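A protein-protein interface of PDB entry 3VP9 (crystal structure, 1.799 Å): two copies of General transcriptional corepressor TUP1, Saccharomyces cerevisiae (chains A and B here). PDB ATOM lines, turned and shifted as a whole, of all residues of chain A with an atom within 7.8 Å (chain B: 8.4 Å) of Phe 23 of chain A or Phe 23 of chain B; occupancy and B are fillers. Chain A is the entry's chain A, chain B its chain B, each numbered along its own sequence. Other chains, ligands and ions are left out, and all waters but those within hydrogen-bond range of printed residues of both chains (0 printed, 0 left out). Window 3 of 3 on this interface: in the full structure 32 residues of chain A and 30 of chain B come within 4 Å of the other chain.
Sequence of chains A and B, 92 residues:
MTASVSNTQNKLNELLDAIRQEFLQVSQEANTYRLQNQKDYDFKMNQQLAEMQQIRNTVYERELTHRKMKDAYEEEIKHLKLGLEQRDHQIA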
ATOM      1  N   ASP A  17     -16.657 -23.535  -0.305  1.00  0.00           N
ATOM      2  CA  ASP A  17     -17.347 -24.823  -0.385  1.00  0.00           C
ATOM      3  C   ASP A  17     -18.648 -24.846   0.419  1.00  0.00           C
ATOM      4  O   ASP A  17     -18.826 -25.659   1.325  1.00  0.00           O
ATOM      5  CB  ASP A  17     -16.421 -25.963   0.042  1.00  0.00           C
ATOM      6  CG  ASP A  17     -15.588 -26.492  -1.110  1.00  0.00           C
ATOM      7  OD1 ASP A  17     -15.079 -27.629  -1.012  1.00  0.00           O
ATOM      8  OD2 ASP A  17     -15.449 -25.770  -2.124  1.00  0.00           O
ATOM      9  N   ALA A  18     -19.553 -23.943   0.054  1.00  0.00           N
ATOM     10  CA  ALA A  18     -20.877 -23.810   0.653  1.00  0.00           C
ATOM     11  C   ALA A  18     -21.451 -22.528   0.091  1.00  0.00           C
ATOM     12  O   ALA A  18     -22.600 -22.162   0.346  1.00  0.00           O
ATOM     13  CB  ALA A  18     -20.778 -23.723   2.169  1.00  0.00           C
ATOM     14  N   ILE A  19     -20.620 -21.860  -0.699  1.00  0.00           N
ATOM     15  CA  ILE A  19     -20.882 -20.502  -1.154  1.00  0.00           C
ATOM     16  C   ILE A  19     -21.457 -20.417  -2.575  1.00  0.00           C
ATOM     17  O   ILE A  19     -21.913 -19.359  -3.001  1.00  0.00           O
ATOM     18  CB  ILE A  19     -19.617 -19.623  -0.994  1.00  0.00           C
ATOM     19  CG1 ILE A  19     -18.384 -20.500  -0.746  1.00  0.00           C
ATOM     20  CG2 ILE A  19     -19.783 -18.695   0.194  1.00  0.00           C
ATOM     21  CD1 ILE A  19     -17.578 -20.813  -1.988  1.00  0.00           C
ATOM     22  N   ARG A  20     -21.416 -21.526  -3.307  1.00  0.00           N
ATOM     23  CA  ARG A  20     -22.259 -21.716  -4.488  1.00  0.00           C
ATOM     24  C   ARG A  20     -22.798 -23.124  -4.314  1.00  0.00           C
ATOM     25  O   ARG A  20     -23.383 -23.714  -5.229  1.00  0.00           O
ATOM     26  CB  ARG A  20     -21.474 -21.578  -5.802  1.00  0.00           C
ATOM     27  CG  ARG A  20     -22.327 -21.073  -6.970  1.00  0.00           C
ATOM     28  CD  ARG A  20     -22.158 -21.905  -8.240  1.00  0.00           C
ATOM     29  NE  ARG A  20     -21.892 -23.316  -7.966  1.00  0.00           N
ATOM     30  CZ  ARG A  20     -20.754 -23.930  -8.274  1.00  0.00           C
ATOM     31  NH1 ARG A  20     -19.779 -23.257  -8.872  1.00  0.00           N
ATOM     32  NH2 ARG A  20     -20.587 -25.215  -7.990  1.00  0.00           N
ATOM     33  N   GLN A  21     -22.593 -23.637  -3.101  1.00  0.00           N
ATOM     34  CA  GLN A  21     -22.877 -25.020  -2.741  1.00  0.00           C
ATOM     35  C   GLN A  21     -24.012 -25.107  -1.723  1.00  0.00           C
ATOM     36  O   GLN A  21     -24.851 -26.005  -1.797  1.00  0.00           O
ATOM     37  CB  GLN A  21     -21.624 -25.676  -2.167  1.00  0.00           C
ATOM     38  CG  GLN A  21     -21.810 -27.124  -1.755  1.00  0.00           C
ATOM     39  CD  GLN A  21     -21.829 -28.083  -2.933  1.00  0.00           C
ATOM     40  OE1 GLN A  21     -22.288 -27.741  -4.024  1.00  0.00           O
ATOM     41  NE2 GLN A  21     -21.317 -29.291  -2.718  1.00  0.00           N
ATOM     42  N   GLU A  22     -24.015 -24.205  -0.743  1.00  0.00           N
ATOM     43  CA  GLU A  22     -25.216 -23.987   0.060  1.00  0.00           C
ATOM     44  C   GLU A  22     -25.920 -22.792  -0.553  1.00  0.00           C
ATOM     45  O   GLU A  22     -27.013 -22.406  -0.139  1.00  0.00           O
ATOM     46  CB  GLU A  22     -24.903 -23.787   1.545  1.00  0.00           C
ATOM     47  CG  GLU A  22     -24.321 -25.015   2.232  1.00  0.00           C
ATOM     48  CD  GLU A  22     -25.043 -25.373   3.519  1.00  0.00           C
ATOM     49  OE1 GLU A  22     -24.719 -26.427   4.110  1.00  0.00           O
ATOM     50  OE2 GLU A  22     -25.935 -24.603   3.939  1.00  0.00           O
ATOM     51  N   PHE A  23     -25.253 -22.204  -1.539  1.00  0.00           N
ATOM     52  CA  PHE A  23     -25.902 -21.333  -2.498  1.00  0.00           C
ATOM     53  C   PHE A  23     -26.351 -22.243  -3.635  1.00  0.00           C
ATOM     54  O   PHE A  23     -26.777 -21.784  -4.697  1.00  0.00           O
ATOM     55  CB  PHE A  23     -24.926 -20.284  -3.009  1.00  0.00           C
ATOM     56  CG  PHE A  23     -25.578 -19.170  -3.757  1.00  0.00           C
ATOM     57  CD1 PHE A  23     -26.139 -18.105  -3.077  1.00  0.00           C
ATOM     58  CD2 PHE A  23     -25.629 -19.181  -5.141  1.00  0.00           C
ATOM     59  CE1 PHE A  23     -26.742 -17.072  -3.760  1.00  0.00           C
ATOM     60  CE2 PHE A  23     -26.232 -18.152  -5.830  1.00  0.00           C
ATOM     61  CZ  PHE A  23     -26.790 -17.096  -5.137  1.00  0.00           C
ATOM     62  N   LEU A  24     -26.218 -23.546  -3.401  1.00  0.00           N
ATOM     63  CA  LEU A  24     -26.831 -24.560  -4.243  1.00  0.00           C
ATOM     64  C   LEU A  24     -27.998 -25.138  -3.453  1.00  0.00           C
ATOM     65  O   LEU A  24     -29.116 -25.239  -3.957  1.00  0.00           O
ATOM     66  CB  LEU A  24     -25.822 -25.652  -4.601  1.00  0.00           C
ATOM     67  CG  LEU A  24     -25.867 -26.199  -6.032  1.00  0.00           C
ATOM     68  CD1 LEU A  24     -24.494 -26.115  -6.697  1.00  0.00           C
ATOM     69  CD2 LEU A  24     -26.391 -27.627  -6.045  1.00  0.00           C
ATOM     70  N   GLN A  25     -27.736 -25.489  -2.197  1.00  0.00           N
ATOM     71  CA  GLN A  25     -28.774 -25.989  -1.307  1.00  0.00           C
ATOM     72  C   GLN A  25     -29.608 -24.833  -0.751  1.00  0.00           C
ATOM     73  O   GLN A  25     -29.972 -24.822   0.425  1.00  0.00           O
ATOM     74  CB  GLN A  25     -28.162 -26.825  -0.178  1.00  0.00           C
ATOM     75  CG  GLN A  25     -29.152 -27.755   0.503  1.00  0.00           C
ATOM     76  CD  GLN A  25     -28.503 -29.016   1.045  1.00  0.00           C
ATOM     77  OE1 GLN A  25     -27.403 -28.977   1.596  1.00  0.00           O
ATOM     78  NE2 GLN A  25     -29.183 -30.148   0.881  1.00  0.00           N
ATOM     79  N   VAL A  26     -29.906 -23.865  -1.615  1.00  0.00           N
ATOM     80  CA  VAL A  26     -30.742 -22.721  -1.264  1.00  0.00           C
ATOM     81  C   VAL A  26     -31.307 -22.068  -2.526  1.00  0.00           C
ATOM     82  O   VAL A  26     -32.395 -21.494  -2.505  1.00  0.00           O
ATOM     83  CB  VAL A  26     -29.960 -21.676  -0.433  1.00  0.00           C
ATOM     84  CG1 VAL A  26     -29.848 -20.356  -1.190  1.00  0.00           C
ATOM     85  CG2 VAL A  26     -30.624 -21.470   0.924  1.00  0.00           C
ATOM     86  N   SER A  27     -30.557 -22.169  -3.621  1.00  0.00           N
ATOM     87  CA  SER A  27     -30.978 -21.633  -4.911  1.00  0.00           C
ATOM     88  C   SER A  27     -31.984 -22.569  -5.556  1.00  0.00           C
ATOM     89  O   SER A  27     -32.577 -22.256  -6.591  1.00  0.00           O
ATOM     90  CB  SER A  27     -29.769 -21.474  -5.835  1.00  0.00           C
ATOM     91  OG  SER A  27     -29.537 -20.116  -6.153  1.00  0.00           O
ATOM     92  N   GLN A  28     -32.171 -23.727  -4.935  1.00  0.00           N
ATOM     93  CA  GLN A  28     -33.037 -24.756  -5.486  1.00  0.00           C
ATOM     94  C   GLN A  28     -34.201 -25.061  -4.549  1.00  0.00           C
ATOM     95  O   GLN A  28     -35.301 -25.387  -5.006  1.00  0.00           O
ATOM     96  CB  GLN A  28     -32.214 -25.995  -5.821  1.00  0.00           C
ATOM     97  CG  GLN A  28     -31.169 -25.701  -6.896  1.00  0.00           C
ATOM     98  CD  GLN A  28     -29.888 -26.491  -6.714  1.00  0.00           C
ATOM     99  OE1 GLN A  28     -29.812 -27.399  -5.882  1.00  0.00           O
ATOM    100  NE2 GLN A  28     -28.869 -26.147  -7.495  1.00  0.00           N
ATOM    101  N   LEU B  16     -18.613 -11.928   3.610  1.00  0.00           N
ATOM    102  CA  LEU B  16     -19.961 -12.472   3.787  1.00  0.00           C
ATOM    103  C   LEU B  16     -20.844 -11.260   3.955  1.00  0.00           C
ATOM    104  O   LEU B  16     -21.631 -11.155   4.903  1.00  0.00           O
ATOM    105  CB  LEU B  16     -20.046 -13.360   5.027  1.00  0.00           C
ATOM    106  CG  LEU B  16     -20.113 -14.867   4.775  1.00  0.00           C
ATOM    107  CD1 LEU B  16     -19.978 -15.633   6.080  1.00  0.00           C
ATOM    108  CD2 LEU B  16     -21.402 -15.242   4.059  1.00  0.00           C
ATOM    109  N   ASP B  17     -20.707 -10.349   3.002  1.00  0.00           N
ATOM    110  CA  ASP B  17     -21.140  -8.977   3.146  1.00  0.00           C
ATOM    111  C   ASP B  17     -21.102  -8.442   1.735  1.00  0.00           C
ATOM    112  O   ASP B  17     -21.302  -7.251   1.466  1.00  0.00           O
ATOM    113  CB  ASP B  17     -20.177  -8.226   4.051  1.00  0.00           C
ATOM    114  CG  ASP B  17     -20.831  -7.771   5.326  1.00  0.00           C
ATOM    115  OD1 ASP B  17     -20.550  -8.352   6.398  1.00  0.00           O
ATOM    116  OD2 ASP B  17     -21.644  -6.829   5.253  1.00  0.00           O
ATOM    117  N   ALA B  18     -20.752  -9.355   0.845  1.00  0.00           N
ATOM    118  CA  ALA B  18     -21.109  -9.294  -0.550  1.00  0.00           C
ATOM    119  C   ALA B  18     -21.781 -10.640  -0.697  1.00  0.00           C
ATOM    120  O   ALA B  18     -22.686 -10.831  -1.509  1.00  0.00           O
ATOM    121  CB  ALA B  18     -19.878  -9.219  -1.411  1.00  0.00           C
ATOM    122  N   ILE B  19     -21.328 -11.565   0.147  1.00  0.00           N
ATOM    123  CA  ILE B  19     -21.801 -12.942   0.166  1.00  0.00           C
ATOM    124  C   ILE B  19     -23.075 -13.127   0.993  1.00  0.00           C
ATOM    125  O   ILE B  19     -23.894 -13.984   0.677  1.00  0.00           O
ATOM    126  CB  ILE B  19     -20.715 -13.905   0.702  1.00  0.00           C
ATOM    127  CG1 ILE B  19     -19.394 -13.691  -0.038  1.00  0.00           C
ATOM    128  CG2 ILE B  19     -21.174 -15.340   0.582  1.00  0.00           C
ATOM    129  CD1 ILE B  19     -19.554 -13.454  -1.522  1.00  0.00           C
ATOM    130  N   ARG B  20     -23.245 -12.346   2.056  1.00  0.00           N
ATOM    131  CA  ARG B  20     -24.486 -12.405   2.825  1.00  0.00           C
ATOM    132  C   ARG B  20     -25.596 -11.884   1.939  1.00  0.00           C
ATOM    133  O   ARG B  20     -26.705 -12.421   1.916  1.00  0.00           O
ATOM    134  CB  ARG B  20     -24.387 -11.566   4.098  1.00  0.00           C
ATOM    135  CG  ARG B  20     -24.855 -12.281   5.358  1.00  0.00           C
ATOM    136  CD  ARG B  20     -24.353 -11.575   6.611  1.00  0.00           C
ATOM    137  NE  ARG B  20     -23.091 -12.131   7.095  1.00  0.00           N
ATOM    138  CZ  ARG B  20     -22.995 -12.998   8.100  1.00  0.00           C
ATOM    139  NH1 ARG B  20     -24.088 -13.405   8.731  1.00  0.00           N
ATOM    140  NH2 ARG B  20     -21.808 -13.455   8.478  1.00  0.00           N
ATOM    141  N   GLN B  21     -25.279 -10.821   1.209  1.00  0.00           N
ATOM    142  CA  GLN B  21     -26.200 -10.274   0.227  1.00  0.00           C
ATOM    143  C   GLN B  21     -25.996 -10.970  -1.122  1.00  0.00           C
ATOM    144  O   GLN B  21     -26.214 -10.384  -2.187  1.00  0.00           O
ATOM    145  CB  GLN B  21     -26.055  -8.753   0.133  1.00  0.00           C
ATOM    146  CG  GLN B  21     -26.451  -8.024   1.425  1.00  0.00           C
ATOM    147  CD  GLN B  21     -27.916  -7.617   1.447  1.00  0.00           C
ATOM    148  OE1 GLN B  21     -28.338  -6.739   0.691  1.00  0.00           O
ATOM    149  NE2 GLN B  21     -28.695  -8.248   2.320  1.00  0.00           N
ATOM    150  N   GLU B  22     -25.542 -12.220  -1.057  1.00  0.00           N
ATOM    151  CA  GLU B  22     -25.716 -13.171  -2.141  1.00  0.00           C
ATOM    152  C   GLU B  22     -26.957 -13.950  -1.744  1.00  0.00           C
ATOM    153  O   GLU B  22     -27.984 -13.917  -2.419  1.00  0.00           O
ATOM    154  CB  GLU B  22     -24.528 -14.140  -2.237  1.00  0.00           C
ATOM    155  CG  GLU B  22     -23.276 -13.607  -2.921  1.00  0.00           C
ATOM    156  CD  GLU B  22     -22.310 -14.715  -3.327  1.00  0.00           C
ATOM    157  OE1 GLU B  22     -22.269 -15.752  -2.630  1.00  0.00           O
ATOM    158  OE2 GLU B  22     -21.612 -14.559  -4.356  1.00  0.00           O
ATOM    159  N   PHE B  23     -26.842 -14.622  -0.605  1.00  0.00           N
ATOM    160  CA  PHE B  23     -27.899 -15.431  -0.026  1.00  0.00           C
ATOM    161  C   PHE B  23     -29.183 -14.651   0.228  1.00  0.00           C
ATOM    162  O   PHE B  23     -30.274 -15.222   0.207  1.00  0.00           O
ATOM    163  CB  PHE B  23     -27.402 -16.066   1.273  1.00  0.00           C
ATOM    164  CG  PHE B  23     -26.380 -17.140   1.059  1.00  0.00           C
ATOM    165  CD1 PHE B  23     -25.228 -16.888   0.331  1.00  0.00           C
ATOM    166  CD2 PHE B  23     -26.574 -18.405   1.581  1.00  0.00           C
ATOM    167  CE1 PHE B  23     -24.290 -17.879   0.126  1.00  0.00           C
ATOM    168  CE2 PHE B  23     -25.640 -19.402   1.383  1.00  0.00           C
ATOM    169  CZ  PHE B  23     -24.496 -19.140   0.655  1.00  0.00           C
ATOM    170  N   LEU B  24     -29.071 -13.352   0.479  1.00  0.00           N
ATOM    171  CA  LEU B  24     -30.285 -12.558   0.680  1.00  0.00           C
ATOM    172  C   LEU B  24     -30.778 -11.861  -0.585  1.00  0.00           C
ATOM    173  O   LEU B  24     -31.420 -10.812  -0.529  1.00  0.00           O
ATOM    174  CB  LEU B  24     -30.175 -11.612   1.881  1.00  0.00           C
ATOM    175  CG  LEU B  24     -30.488 -12.292   3.226  1.00  0.00           C
ATOM    176  CD1 LEU B  24     -30.531 -13.810   3.081  1.00  0.00           C
ATOM    177  CD2 LEU B  24     -29.491 -11.877   4.301  1.00  0.00           C
ATOM    178  N   GLN B  25     -30.439 -12.453  -1.727  1.00  0.00           N
ATOM    179  CA  GLN B  25     -31.269 -12.352  -2.919  1.00  0.00           C
ATOM    180  C   GLN B  25     -31.493 -13.748  -3.473  1.00  0.00           C
ATOM    181  O   GLN B  25     -31.275 -14.004  -4.663  1.00  0.00           O
ATOM    182  CB  GLN B  25     -30.710 -11.439  -4.009  1.00  0.00           C
ATOM    183  CG  GLN B  25     -31.792 -11.087  -5.057  1.00  0.00           C
ATOM    184  CD  GLN B  25     -31.275 -11.119  -6.486  1.00  0.00           C
ATOM    185  OE1 GLN B  25     -30.302 -10.443  -6.813  1.00  0.00           O
ATOM    186  NE2 GLN B  25     -31.934 -11.897  -7.348  1.00  0.00           N
ATOM    187  N   VAL B  26     -31.857 -14.663  -2.584  1.00  0.00           N
ATOM    188  CA  VAL B  26     -32.556 -15.866  -2.973  1.00  0.00           C
ATOM    189  C   VAL B  26     -33.844 -15.822  -2.174  1.00  0.00           C
ATOM    190  O   VAL B  26     -34.931 -15.984  -2.714  1.00  0.00           O
ATOM    191  CB  VAL B  26     -31.772 -17.141  -2.630  1.00  0.00           C
ATOM    192  CG1 VAL B  26     -32.009 -18.205  -3.700  1.00  0.00           C
ATOM    193  CG2 VAL B  26     -30.294 -16.827  -2.511  1.00  0.00           C
ATOM    194  N   SER B  27     -33.705 -15.554  -0.879  1.00  0.00           N
ATOM    195  CA  SER B  27     -34.850 -15.461   0.020  1.00  0.00           C
ATOM    196  C   SER B  27     -35.551 -14.109  -0.066  1.00  0.00           C
ATOM    197  O   SER B  27     -36.735 -14.001   0.253  1.00  0.00           O
ATOM    198  CB  SER B  27     -34.436 -15.765   1.462  1.00  0.00           C
ATOM    199  OG  SER B  27     -34.068 -17.130   1.605  1.00  0.00           O
ATOM    200  N   GLN B  28     -34.825 -13.079  -0.490  1.00  0.00           N
ATOM    201  CA  GLN B  28     -35.452 -11.797  -0.787  1.00  0.00           C
ATOM    202  C   GLN B  28     -35.867 -11.840  -2.252  1.00  0.00           C
ATOM    203  O   GLN B  28     -36.212 -10.822  -2.855  1.00  0.00           O
ATOM    204  CB  GLN B  28     -34.505 -10.630  -0.500  1.00  0.00           C
ATOM    205  CG  GLN B  28     -35.188  -9.263  -0.449  1.00  0.00           C
ATOM    206  CD  GLN B  28     -34.363  -8.231   0.299  1.00  0.00           C
ATOM    207  OE1 GLN B  28     -33.571  -8.574   1.178  1.00  0.00           O
ATOM    208  NE2 GLN B  28     -34.544  -6.961  -0.046  1.00  0.00           N
ATOM    209  N   GLU B  29     -35.831 -13.049  -2.808  1.00  0.00           N
ATOM    210  CA  GLU B  29     -36.252 -13.305  -4.175  1.00  0.00           C
ATOM    211  C   GLU B  29     -37.441 -14.262  -4.140  1.00  0.00           C
ATOM    212  O   GLU B  29     -38.428 -14.070  -4.844  1.00  0.00           O
ATOM    213  CB  GLU B  29     -35.104 -13.920  -4.981  1.00  0.00           C
ATOM    214  CG  GLU B  29     -35.076 -13.494  -6.439  1.00  0.00           C
ATOM    215  CD  GLU B  29     -34.263 -14.429  -7.316  1.00  0.00           C
ATOM    216  OE1 GLU B  29     -34.882 -15.226  -8.056  1.00  0.00           O
ATOM    217  OE2 GLU B  29     -33.015 -14.365  -7.275  1.00  0.00           O
ATOM    218  N   ALA B  30     -37.341 -15.291  -3.304  1.00  0.00           N
ATOM    219  CA  ALA B  30     -38.414 -16.265  -3.153  1.00  0.00           C
ATOM    220  C   ALA B  30     -39.651 -15.592  -2.574  1.00  0.00           C
ATOM    221  O   ALA B  30     -40.782 -15.983  -2.866  1.00  0.00           O
ATOM    222  CB  ALA B  30     -37.969 -17.413  -2.263  1.00  0.00           C
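Ala 18 of chain A touches Phe 23 of chain B, but with the chains exchanged Phe 23 of chain A does not touch Ala 18 of chain B (7.8 Å). Ile 19 of chain A touches Glu 22 of chain B, but with the chains exchanged Glu 22 of chain A does not touch Ile 19 of chain B (8.9 Å). Glu 22 of chain A touches Phe 23 of chain B, and with the chains exchanged Phe 23 of chain A touches Glu 22 of chain B. Phe 23 of chain A touches Val 26 of chain B, but with the chains exchanged Val 26 of chain A does not touch Phe 23 of chain B (4.7 Å). Positions printed for both chains: 17, 18, 19, 20, 21, 22, 23, 24, 25, 26, 27 and 28. Of the 9 pairs that touch across the chains among the printed residues, 5 have their exchanged pair printed and touching as well.
Of the 15 printed residues of chain B, 4 touch a printed residue of chain A. Hydrophobic or aromatic side chains of chain B that line the printed part of chain A: Ile 19, Phe 23 and Val 26. Hydrophobic or aromatic side chains of chain A within 4 Å of the printed part of chain B: Ile 19, Phe 23 and Val 26. Along chain A the printed residues that touch a printed residue of chain B span positions 18 to 27.
N of Phe 23 of chain A lies within hydrogen-bond range of O of Ala 18 of chain A (3.3 Å).
Among the printed residues, pairs that only touch across the chains: Val 26 of chain A with Val 26 of chain B, Ala 18 of chain A with Phe 23 of chain B, Glu 22 of chain A with Phe 23 of chain B, Ile 19 of chain A with Glu 22 of chain B, Phe 23 of chain A with Glu 22 of chain B, Ile 19 of chain A with Ile 19 of chain B, Phe 23 of chain A with Phe 23 of chain B, Phe 23 of chain A with Val 26 of chain B and Ser 27 of chain A with Val 26 of chain B.
Printed residues of chain B within 4 Å of Ala 18 of chain A: Phe 23. Printed residues of chain B within 4 Å of Ile 19 of chain A: Ile 19 (3.7 Å) and Glu 22 (3.6 Å). Phe 23 of chain A touches just these residues of chain B: Glu 22 (3.6 Å), Phe 23 (3.7 Å) and Val 26 (3.8 Å). Printed residues of chain B within 4 Å of Ser 27 of chain A: Val 26. Of the printed residues of chain A, Ile 19 of chain B touches Ile 19 (3.7 Å). Arg 20 of chain B touches none of the printed residues of chain A. Phe 23 of chain B touches just these residues of chain A: Ala 18, Glu 22 and Phe 23. Gln 25 of chain B touches none of the printed residues of chain A. Of the printed residues of chain A, Val 26 of chain B touches Phe 23 (3.8 Å), Val 26 (3.5 Å) and Ser 27 (3.8 Å). The nearest residue of chain A that does not touch Phe 23 of chain B is Ile 19 of chain A (4.2 Å).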
